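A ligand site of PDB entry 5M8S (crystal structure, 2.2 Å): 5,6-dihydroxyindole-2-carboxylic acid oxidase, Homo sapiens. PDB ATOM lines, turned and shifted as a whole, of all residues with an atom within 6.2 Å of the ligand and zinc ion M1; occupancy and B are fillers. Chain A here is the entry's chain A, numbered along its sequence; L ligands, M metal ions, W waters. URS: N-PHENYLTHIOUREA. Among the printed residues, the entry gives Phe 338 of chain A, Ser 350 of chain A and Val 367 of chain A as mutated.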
ATOM      1  N   HIS A 168     -13.218  -0.209   9.686  1.00  0.00           N
ATOM      2  CA  HIS A 168     -13.434  -0.494  11.102  1.00  0.00           C
ATOM      3  C   HIS A 168     -14.798   0.022  11.532  1.00  0.00           C
ATOM      4  O   HIS A 168     -15.571  -0.695  12.190  1.00  0.00           O
ATOM      5  CB  HIS A 168     -12.326   0.159  11.932  1.00  0.00           C
ATOM      6  CG  HIS A 168     -12.187  -0.349  13.344  1.00  0.00           C
ATOM      7  ND1 HIS A 168     -12.840   0.237  14.423  1.00  0.00           N
ATOM      8  CD2 HIS A 168     -11.437  -1.349  13.858  1.00  0.00           C
ATOM      9  CE1 HIS A 168     -12.483  -0.395  15.530  1.00  0.00           C
ATOM     10  NE2 HIS A 168     -11.631  -1.357  15.218  1.00  0.00           N
ATOM     11  N   HIS A 191     -15.203  -7.249  17.058  1.00  0.00           N
ATOM     12  CA  HIS A 191     -14.893  -7.232  18.480  1.00  0.00           C
ATOM     13  C   HIS A 191     -15.855  -8.144  19.204  1.00  0.00           C
ATOM     14  O   HIS A 191     -16.869  -8.581  18.646  1.00  0.00           O
ATOM     15  CB  HIS A 191     -14.997  -5.829  19.078  1.00  0.00           C
ATOM     16  CG  HIS A 191     -14.229  -4.810  18.318  1.00  0.00           C
ATOM     17  ND1 HIS A 191     -14.697  -4.228  17.155  1.00  0.00           N
ATOM     18  CD2 HIS A 191     -12.973  -4.319  18.496  1.00  0.00           C
ATOM     19  CE1 HIS A 191     -13.796  -3.379  16.692  1.00  0.00           C
ATOM     20  NE2 HIS A 191     -12.748  -3.415  17.492  1.00  0.00           N
ATOM     21  N   GLU A 192     -15.546  -8.445  20.460  1.00  0.00           N
ATOM     22  CA  GLU A 192     -16.401  -9.230  21.326  1.00  0.00           C
ATOM     23  C   GLU A 192     -16.723 -10.571  20.676  1.00  0.00           C
ATOM     24  O   GLU A 192     -17.878 -10.965  20.541  1.00  0.00           O
ATOM     25  CB  GLU A 192     -17.665  -8.456  21.669  1.00  0.00           C
ATOM     26  CG  GLU A 192     -17.348  -7.075  22.132  1.00  0.00           C
ATOM     27  CD  GLU A 192     -18.541  -6.311  22.659  1.00  0.00           C
ATOM     28  OE1 GLU A 192     -19.315  -6.880  23.459  1.00  0.00           O
ATOM     29  OE2 GLU A 192     -18.694  -5.120  22.273  1.00  0.00           O
ATOM     30  N   PHE A 196     -11.852 -11.125  16.701  1.00  0.00           N
ATOM     31  CA  PHE A 196     -11.201  -9.863  17.079  1.00  0.00           C
ATOM     32  C   PHE A 196      -9.744  -9.837  16.608  1.00  0.00           C
ATOM     33  O   PHE A 196      -9.308  -8.857  15.993  1.00  0.00           O
ATOM     34  CB  PHE A 196     -11.293  -9.663  18.597  1.00  0.00           C
ATOM     35  CG  PHE A 196     -10.366  -8.613  19.134  1.00  0.00           C
ATOM     36  CD1 PHE A 196     -10.631  -7.270  18.919  1.00  0.00           C
ATOM     37  CD2 PHE A 196      -9.225  -8.962  19.853  1.00  0.00           C
ATOM     38  CE1 PHE A 196      -9.775  -6.272  19.423  1.00  0.00           C
ATOM     39  CE2 PHE A 196      -8.361  -7.975  20.356  1.00  0.00           C
ATOM     40  CZ  PHE A 196      -8.646  -6.628  20.140  1.00  0.00           C
ATOM     41  N   HIS A 200      -8.343  -7.678  13.087  1.00  0.00           N
ATOM     42  CA  HIS A 200      -7.397  -6.565  13.209  1.00  0.00           C
ATOM     43  C   HIS A 200      -6.061  -6.898  12.580  1.00  0.00           C
ATOM     44  O   HIS A 200      -5.365  -6.006  12.098  1.00  0.00           O
ATOM     45  CB  HIS A 200      -7.249  -6.171  14.671  1.00  0.00           C
ATOM     46  CG  HIS A 200      -8.459  -5.492  15.221  1.00  0.00           C
ATOM     47  ND1 HIS A 200      -9.586  -6.185  15.598  1.00  0.00           N
ATOM     48  CD2 HIS A 200      -8.727  -4.186  15.437  1.00  0.00           C
ATOM     49  CE1 HIS A 200     -10.510  -5.336  16.017  1.00  0.00           C
ATOM     50  NE2 HIS A 200     -10.013  -4.115  15.933  1.00  0.00           N
ATOM     51  N   ARG A 297     -13.098   7.727  36.197  1.00  0.00           N
ATOM     52  CA  ARG A 297     -12.926   6.289  36.054  1.00  0.00           C
ATOM     53  C   ARG A 297     -11.473   5.939  36.344  1.00  0.00           C
ATOM     54  O   ARG A 297     -10.693   5.637  35.428  1.00  0.00           O
ATOM     55  CB  ARG A 297     -13.354   5.863  34.658  1.00  0.00           C
ATOM     56  CG  ARG A 297     -13.901   4.496  34.538  1.00  0.00           C
ATOM     57  CD  ARG A 297     -14.589   4.360  33.182  1.00  0.00           C
ATOM     58  NE  ARG A 297     -14.656   2.955  32.803  1.00  0.00           N
ATOM     59  CZ  ARG A 297     -15.094   2.526  31.631  1.00  0.00           C
ATOM     60  NH1 ARG A 297     -15.495   3.397  30.713  1.00  0.00           N
ATOM     61  NH2 ARG A 297     -15.109   1.230  31.378  1.00  0.00           N
ATOM     62  N   PHE A 338     -11.629  -7.881  28.145  1.00  0.00           N
ATOM     63  CA  PHE A 338     -12.858  -8.006  28.930  1.00  0.00           C
ATOM     64  C   PHE A 338     -12.687  -8.869  30.169  1.00  0.00           C
ATOM     65  O   PHE A 338     -13.467  -8.729  31.113  1.00  0.00           O
ATOM     66  CB  PHE A 338     -13.988  -8.557  28.079  1.00  0.00           C
ATOM     67  CG  PHE A 338     -14.468  -7.612  27.031  1.00  0.00           C
ATOM     68  CD1 PHE A 338     -15.250  -6.496  27.387  1.00  0.00           C
ATOM     69  CD2 PHE A 338     -14.164  -7.827  25.690  1.00  0.00           C
ATOM     70  CE1 PHE A 338     -15.721  -5.613  26.429  1.00  0.00           C
ATOM     71  CE2 PHE A 338     -14.614  -6.944  24.712  1.00  0.00           C
ATOM     72  CZ  PHE A 338     -15.408  -5.840  25.086  1.00  0.00           C
ATOM     73  N   SER A 350     -11.367  -3.716  32.898  1.00  0.00           N
ATOM     74  CA  SER A 350     -10.793  -3.268  31.618  1.00  0.00           C
ATOM     75  C   SER A 350      -9.302  -3.516  31.685  1.00  0.00           C
ATOM     76  O   SER A 350      -8.601  -2.915  32.492  1.00  0.00           O
ATOM     77  CB  SER A 350     -11.074  -1.793  31.337  1.00  0.00           C
ATOM     78  OG  SER A 350     -12.343  -1.642  30.737  1.00  0.00           O
ATOM     79  N   HIS A 353      -5.780  -4.601  25.815  1.00  0.00           N
ATOM     80  CA  HIS A 353      -6.212  -3.828  24.652  1.00  0.00           C
ATOM     81  C   HIS A 353      -7.327  -2.852  24.989  1.00  0.00           C
ATOM     82  O   HIS A 353      -7.266  -1.666  24.629  1.00  0.00           O
ATOM     83  CB  HIS A 353      -6.637  -4.781  23.537  1.00  0.00           C
ATOM     84  CG  HIS A 353      -7.590  -4.182  22.537  1.00  0.00           C
ATOM     85  ND1 HIS A 353      -8.957  -4.259  22.674  1.00  0.00           N
ATOM     86  CD2 HIS A 353      -7.361  -3.573  21.351  1.00  0.00           C
ATOM     87  CE1 HIS A 353      -9.538  -3.682  21.640  1.00  0.00           C
ATOM     88  NE2 HIS A 353      -8.586  -3.249  20.828  1.00  0.00           N
ATOM     89  N   ASN A 354      -8.368  -3.328  25.688  1.00  0.00           N
ATOM     90  CA  ASN A 354      -9.467  -2.427  26.021  1.00  0.00           C
ATOM     91  C   ASN A 354      -8.977  -1.285  26.921  1.00  0.00           C
ATOM     92  O   ASN A 354      -9.369  -0.129  26.725  1.00  0.00           O
ATOM     93  CB  ASN A 354     -10.623  -3.182  26.669  1.00  0.00           C
ATOM     94  CG  ASN A 354     -11.490  -3.946  25.651  1.00  0.00           C
ATOM     95  OD1 ASN A 354     -11.364  -3.769  24.435  1.00  0.00           O
ATOM     96  ND2 ASN A 354     -12.398  -4.778  26.138  1.00  0.00           N
ATOM     97  N   LEU A 355      -8.091  -1.593  27.875  1.00  0.00           N
ATOM     98  CA  LEU A 355      -7.573  -0.570  28.773  1.00  0.00           C
ATOM     99  C   LEU A 355      -6.705   0.436  28.033  1.00  0.00           C
ATOM    100  O   LEU A 355      -6.808   1.651  28.287  1.00  0.00           O
ATOM    101  CB  LEU A 355      -6.782  -1.221  29.920  1.00  0.00           C
ATOM    102  CG  LEU A 355      -6.055  -0.335  30.929  1.00  0.00           C
ATOM    103  CD1 LEU A 355      -6.990   0.715  31.593  1.00  0.00           C
ATOM    104  CD2 LEU A 355      -5.356  -1.198  31.979  1.00  0.00           C
ATOM    105  N   HIS A 357      -7.015   1.397  25.013  1.00  0.00           N
ATOM    106  CA  HIS A 357      -7.954   2.270  24.335  1.00  0.00           C
ATOM    107  C   HIS A 357      -8.544   3.296  25.291  1.00  0.00           C
ATOM    108  O   HIS A 357      -8.540   4.508  25.006  1.00  0.00           O
ATOM    109  CB  HIS A 357      -9.081   1.456  23.696  1.00  0.00           C
ATOM    110  CG  HIS A 357      -8.815   0.990  22.293  1.00  0.00           C
ATOM    111  ND1 HIS A 357      -8.782   1.852  21.224  1.00  0.00           N
ATOM    112  CD2 HIS A 357      -8.679  -0.249  21.781  1.00  0.00           C
ATOM    113  CE1 HIS A 357      -8.596   1.165  20.110  1.00  0.00           C
ATOM    114  NE2 HIS A 357      -8.521  -0.111  20.425  1.00  0.00           N
ATOM    115  N   LEU A 358      -9.050   2.840  26.449  1.00  0.00           N
ATOM    116  CA  LEU A 358      -9.704   3.749  27.379  1.00  0.00           C
ATOM    117  C   LEU A 358      -8.708   4.726  28.005  1.00  0.00           C
ATOM    118  O   LEU A 358      -9.089   5.863  28.337  1.00  0.00           O
ATOM    119  CB  LEU A 358     -10.446   2.958  28.461  1.00  0.00           C
ATOM    120  CG  LEU A 358     -11.652   2.155  27.945  1.00  0.00           C
ATOM    121  CD1 LEU A 358     -12.274   1.250  29.019  1.00  0.00           C
ATOM    122  CD2 LEU A 358     -12.722   3.084  27.366  1.00  0.00           C
ATOM    123  N   THR A 363     -10.833  10.371  21.246  1.00  0.00           N
ATOM    124  CA  THR A 363     -11.193   9.761  19.968  1.00  0.00           C
ATOM    125  C   THR A 363     -10.694   8.324  19.865  1.00  0.00           C
ATOM    126  O   THR A 363     -11.420   7.419  19.445  1.00  0.00           O
ATOM    127  CB  THR A 363     -10.603  10.610  18.841  1.00  0.00           C
ATOM    128  OG1 THR A 363     -10.974  11.967  19.054  1.00  0.00           O
ATOM    129  CG2 THR A 363     -11.129  10.152  17.487  1.00  0.00           C
ATOM    130  N   GLY A 364      -9.444   8.084  20.263  1.00  0.00           N
ATOM    131  CA  GLY A 364      -8.888   6.733  20.199  1.00  0.00           C
ATOM    132  C   GLY A 364      -9.516   5.748  21.165  1.00  0.00           C
ATOM    133  O   GLY A 364      -9.194   4.554  21.106  1.00  0.00           O
ATOM    134  N   GLY A 365     -10.407   6.215  22.039  1.00  0.00           N
ATOM    135  CA  GLY A 365     -11.054   5.341  22.985  1.00  0.00           C
ATOM    136  C   GLY A 365     -12.558   5.311  22.821  1.00  0.00           C
ATOM    137  O   GLY A 365     -13.277   4.973  23.761  1.00  0.00           O
ATOM    138  N   GLN A 366     -13.036   5.684  21.626  1.00  0.00           N
ATOM    139  CA  GLN A 366     -14.442   5.640  21.288  1.00  0.00           C
ATOM    140  C   GLN A 366     -14.655   4.626  20.168  1.00  0.00           C
ATOM    141  O   GLN A 366     -13.969   4.688  19.140  1.00  0.00           O
ATOM    142  CB  GLN A 366     -14.954   7.031  20.871  1.00  0.00           C
ATOM    143  CG  GLN A 366     -15.003   8.005  22.027  1.00  0.00           C
ATOM    144  CD  GLN A 366     -15.348   9.421  21.589  1.00  0.00           C
ATOM    145  OE1 GLN A 366     -14.446  10.211  21.256  1.00  0.00           O
ATOM    146  NE2 GLN A 366     -16.615   9.768  21.641  1.00  0.00           N
ATOM    147  N   VAL A 367     -15.637   3.738  20.345  1.00  0.00           N
ATOM    148  CA  VAL A 367     -15.759   2.544  19.507  1.00  0.00           C
ATOM    149  C   VAL A 367     -16.027   2.911  18.043  1.00  0.00           C
ATOM    150  O   VAL A 367     -15.581   2.194  17.135  1.00  0.00           O
ATOM    151  CB  VAL A 367     -16.816   1.571  20.064  1.00  0.00           C
ATOM    152  CG1 VAL A 367     -16.409   1.081  21.437  1.00  0.00           C
ATOM    153  CG2 VAL A 367     -18.222   2.204  20.119  1.00  0.00           C
ATOM    154  N   SER A 370     -12.190   5.088  16.978  1.00  0.00           N
ATOM    155  CA  SER A 370     -10.838   4.897  17.491  1.00  0.00           C
ATOM    156  C   SER A 370      -9.733   4.916  16.436  1.00  0.00           C
ATOM    157  O   SER A 370      -8.695   5.543  16.708  1.00  0.00           O
ATOM    158  CB  SER A 370     -10.797   3.630  18.348  1.00  0.00           C
ATOM    159  OG  SER A 370     -11.250   2.458  17.657  1.00  0.00           O
ATOM    160  N   PHE A 376      -3.962   4.176  17.300  1.00  0.00           N
ATOM    161  CA  PHE A 376      -4.644   2.910  17.022  1.00  0.00           C
ATOM    162  C   PHE A 376      -3.724   1.944  16.272  1.00  0.00           C
ATOM    163  O   PHE A 376      -3.684   0.755  16.604  1.00  0.00           O
ATOM    164  CB  PHE A 376      -5.922   3.182  16.201  1.00  0.00           C
ATOM    165  CG  PHE A 376      -6.702   1.935  15.822  1.00  0.00           C
ATOM    166  CD1 PHE A 376      -6.321   1.151  14.746  1.00  0.00           C
ATOM    167  CD2 PHE A 376      -7.868   1.613  16.497  1.00  0.00           C
ATOM    168  CE1 PHE A 376      -7.036   0.033  14.385  1.00  0.00           C
ATOM    169  CE2 PHE A 376      -8.612   0.503  16.127  1.00  0.00           C
ATOM    170  CZ  PHE A 376      -8.182  -0.297  15.079  1.00  0.00           C
ATOM    171  N   LEU A 379      -1.106   0.620  18.707  1.00  0.00           N
ATOM    172  CA  LEU A 379      -1.791  -0.184  19.707  1.00  0.00           C
ATOM    173  C   LEU A 379      -2.110  -1.568  19.161  1.00  0.00           C
ATOM    174  O   LEU A 379      -1.970  -2.573  19.860  1.00  0.00           O
ATOM    175  CB  LEU A 379      -3.062   0.551  20.144  1.00  0.00           C
ATOM    176  CG  LEU A 379      -3.908   0.072  21.328  1.00  0.00           C
ATOM    177  CD1 LEU A 379      -4.798   1.203  21.806  1.00  0.00           C
ATOM    178  CD2 LEU A 379      -4.796  -1.155  20.950  1.00  0.00           C
ATOM    179  N   HIS A 380      -2.493  -1.655  17.887  1.00  0.00           N
ATOM    180  CA  HIS A 380      -2.908  -2.953  17.366  1.00  0.00           C
ATOM    181  C   HIS A 380      -1.776  -3.769  16.745  1.00  0.00           C
ATOM    182  O   HIS A 380      -1.909  -4.997  16.675  1.00  0.00           O
ATOM    183  CB  HIS A 380      -4.062  -2.824  16.367  1.00  0.00           C
ATOM    184  CG  HIS A 380      -5.398  -2.862  17.033  1.00  0.00           C
ATOM    185  ND1 HIS A 380      -5.954  -4.038  17.502  1.00  0.00           N
ATOM    186  CD2 HIS A 380      -6.235  -1.873  17.402  1.00  0.00           C
ATOM    187  CE1 HIS A 380      -7.108  -3.761  18.084  1.00  0.00           C
ATOM    188  NE2 HIS A 380      -7.299  -2.466  18.035  1.00  0.00           N
HETATM  189  N1  URS L   1     -13.012  -0.022  23.093  1.00  0.00           N
HETATM  190  N2  URS L   1     -13.604   2.125  23.908  1.00  0.00           N
HETATM  191  C1  URS L   1     -15.426  -2.091  25.172  1.00  0.00           C
HETATM  192  C2  URS L   1     -14.751  -1.386  24.008  1.00  0.00           C
HETATM  193  C3  URS L   1     -13.660  -0.690  24.203  1.00  0.00           C
HETATM  194  C4  URS L   1     -13.075  -0.563  25.594  1.00  0.00           C
HETATM  195  C5  URS L   1     -13.648  -1.154  26.611  1.00  0.00           C
HETATM  196  C6  URS L   1     -14.905  -1.975  26.375  1.00  0.00           C
HETATM  197  C7  URS L   1     -13.021   1.430  23.020  1.00  0.00           C
HETATM  198  S1  URS L   1     -12.287   2.128  21.785  1.00  0.00           S
HETATM  199 ZN    ZN M   1      -8.691  -1.812  19.319  1.00  0.00          ZN
HETATM  200 ZN    ZN M   2     -11.044  -2.507  16.749  1.00  0.00          ZN
HETATM  201  O   HOH W   1     -12.290  -1.756  21.171  1.00  0.00           O
HETATM  202  O   HOH W   2     -12.092   0.162  19.320  1.00  0.00           O
HETATM  203  O   HOH W   3     -15.947   1.817  26.000  1.00  0.00           O
HETATM  204  O   HOH W   4     -10.450  -1.436  18.342  1.00  0.00           O
HETATM  205  O   HOH W   5     -15.605  -3.517  21.610  1.00  0.00           O
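Water W2 bridges the side-chain hydroxyl (OG) of Ser 370 and a sulfur (S1) of the ligand.
Zinc ion M1 is bound by NE2 of His 380 (2.0 Å), NE2 of His 357 (2.0 Å), water W4 (2.0 Å) and NE2 of His 353 (2.1 Å).
Zinc ion M1 has four donor atoms within binding distance.
The backbone carbonyl oxygen (O) of Gly 364 lies within hydrogen-bond range of a ring nitrogen (ND1) of His 357 (2.7 Å).
OD1 of Asn 354 sits at hydrogen-bond distance from ND1 of His 353 (3.0 Å).
Phe 338 touches the ligand.
Asn 354 touches the ligand.
CD1 of Leu 358 touches C5 of the ligand (3.7 Å).
Gly 364 touches the ligand.
Val 367 touches the ligand.
Eight residues have an atom within 4 Å of the ligand: Phe 338, Asn 354, His 357, Leu 358, Gly 364, Gly 365, Gln 366 and Val 367.
The nearest printed residue that does not touch the ligand is Ser 370 (4.04 Å).
A ring nitrogen (ND1) of His 357 sits close to a sulfur (S1) of the ligand, 3.6 Å away.
S1 of the ligand sits close to N of Gln 366.
N2 of the ligand is in hydrogen-bond range of O of Gly 365.
Residues that only touch zinc ion M1: Phe 376 (3.9 Å).
Within 4 Å of zinc ion M1: His 353, His 357, Phe 376 and His 380.
The nearest printed residue that does not touch zinc ion M1 is Leu 379 (4.3 Å).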
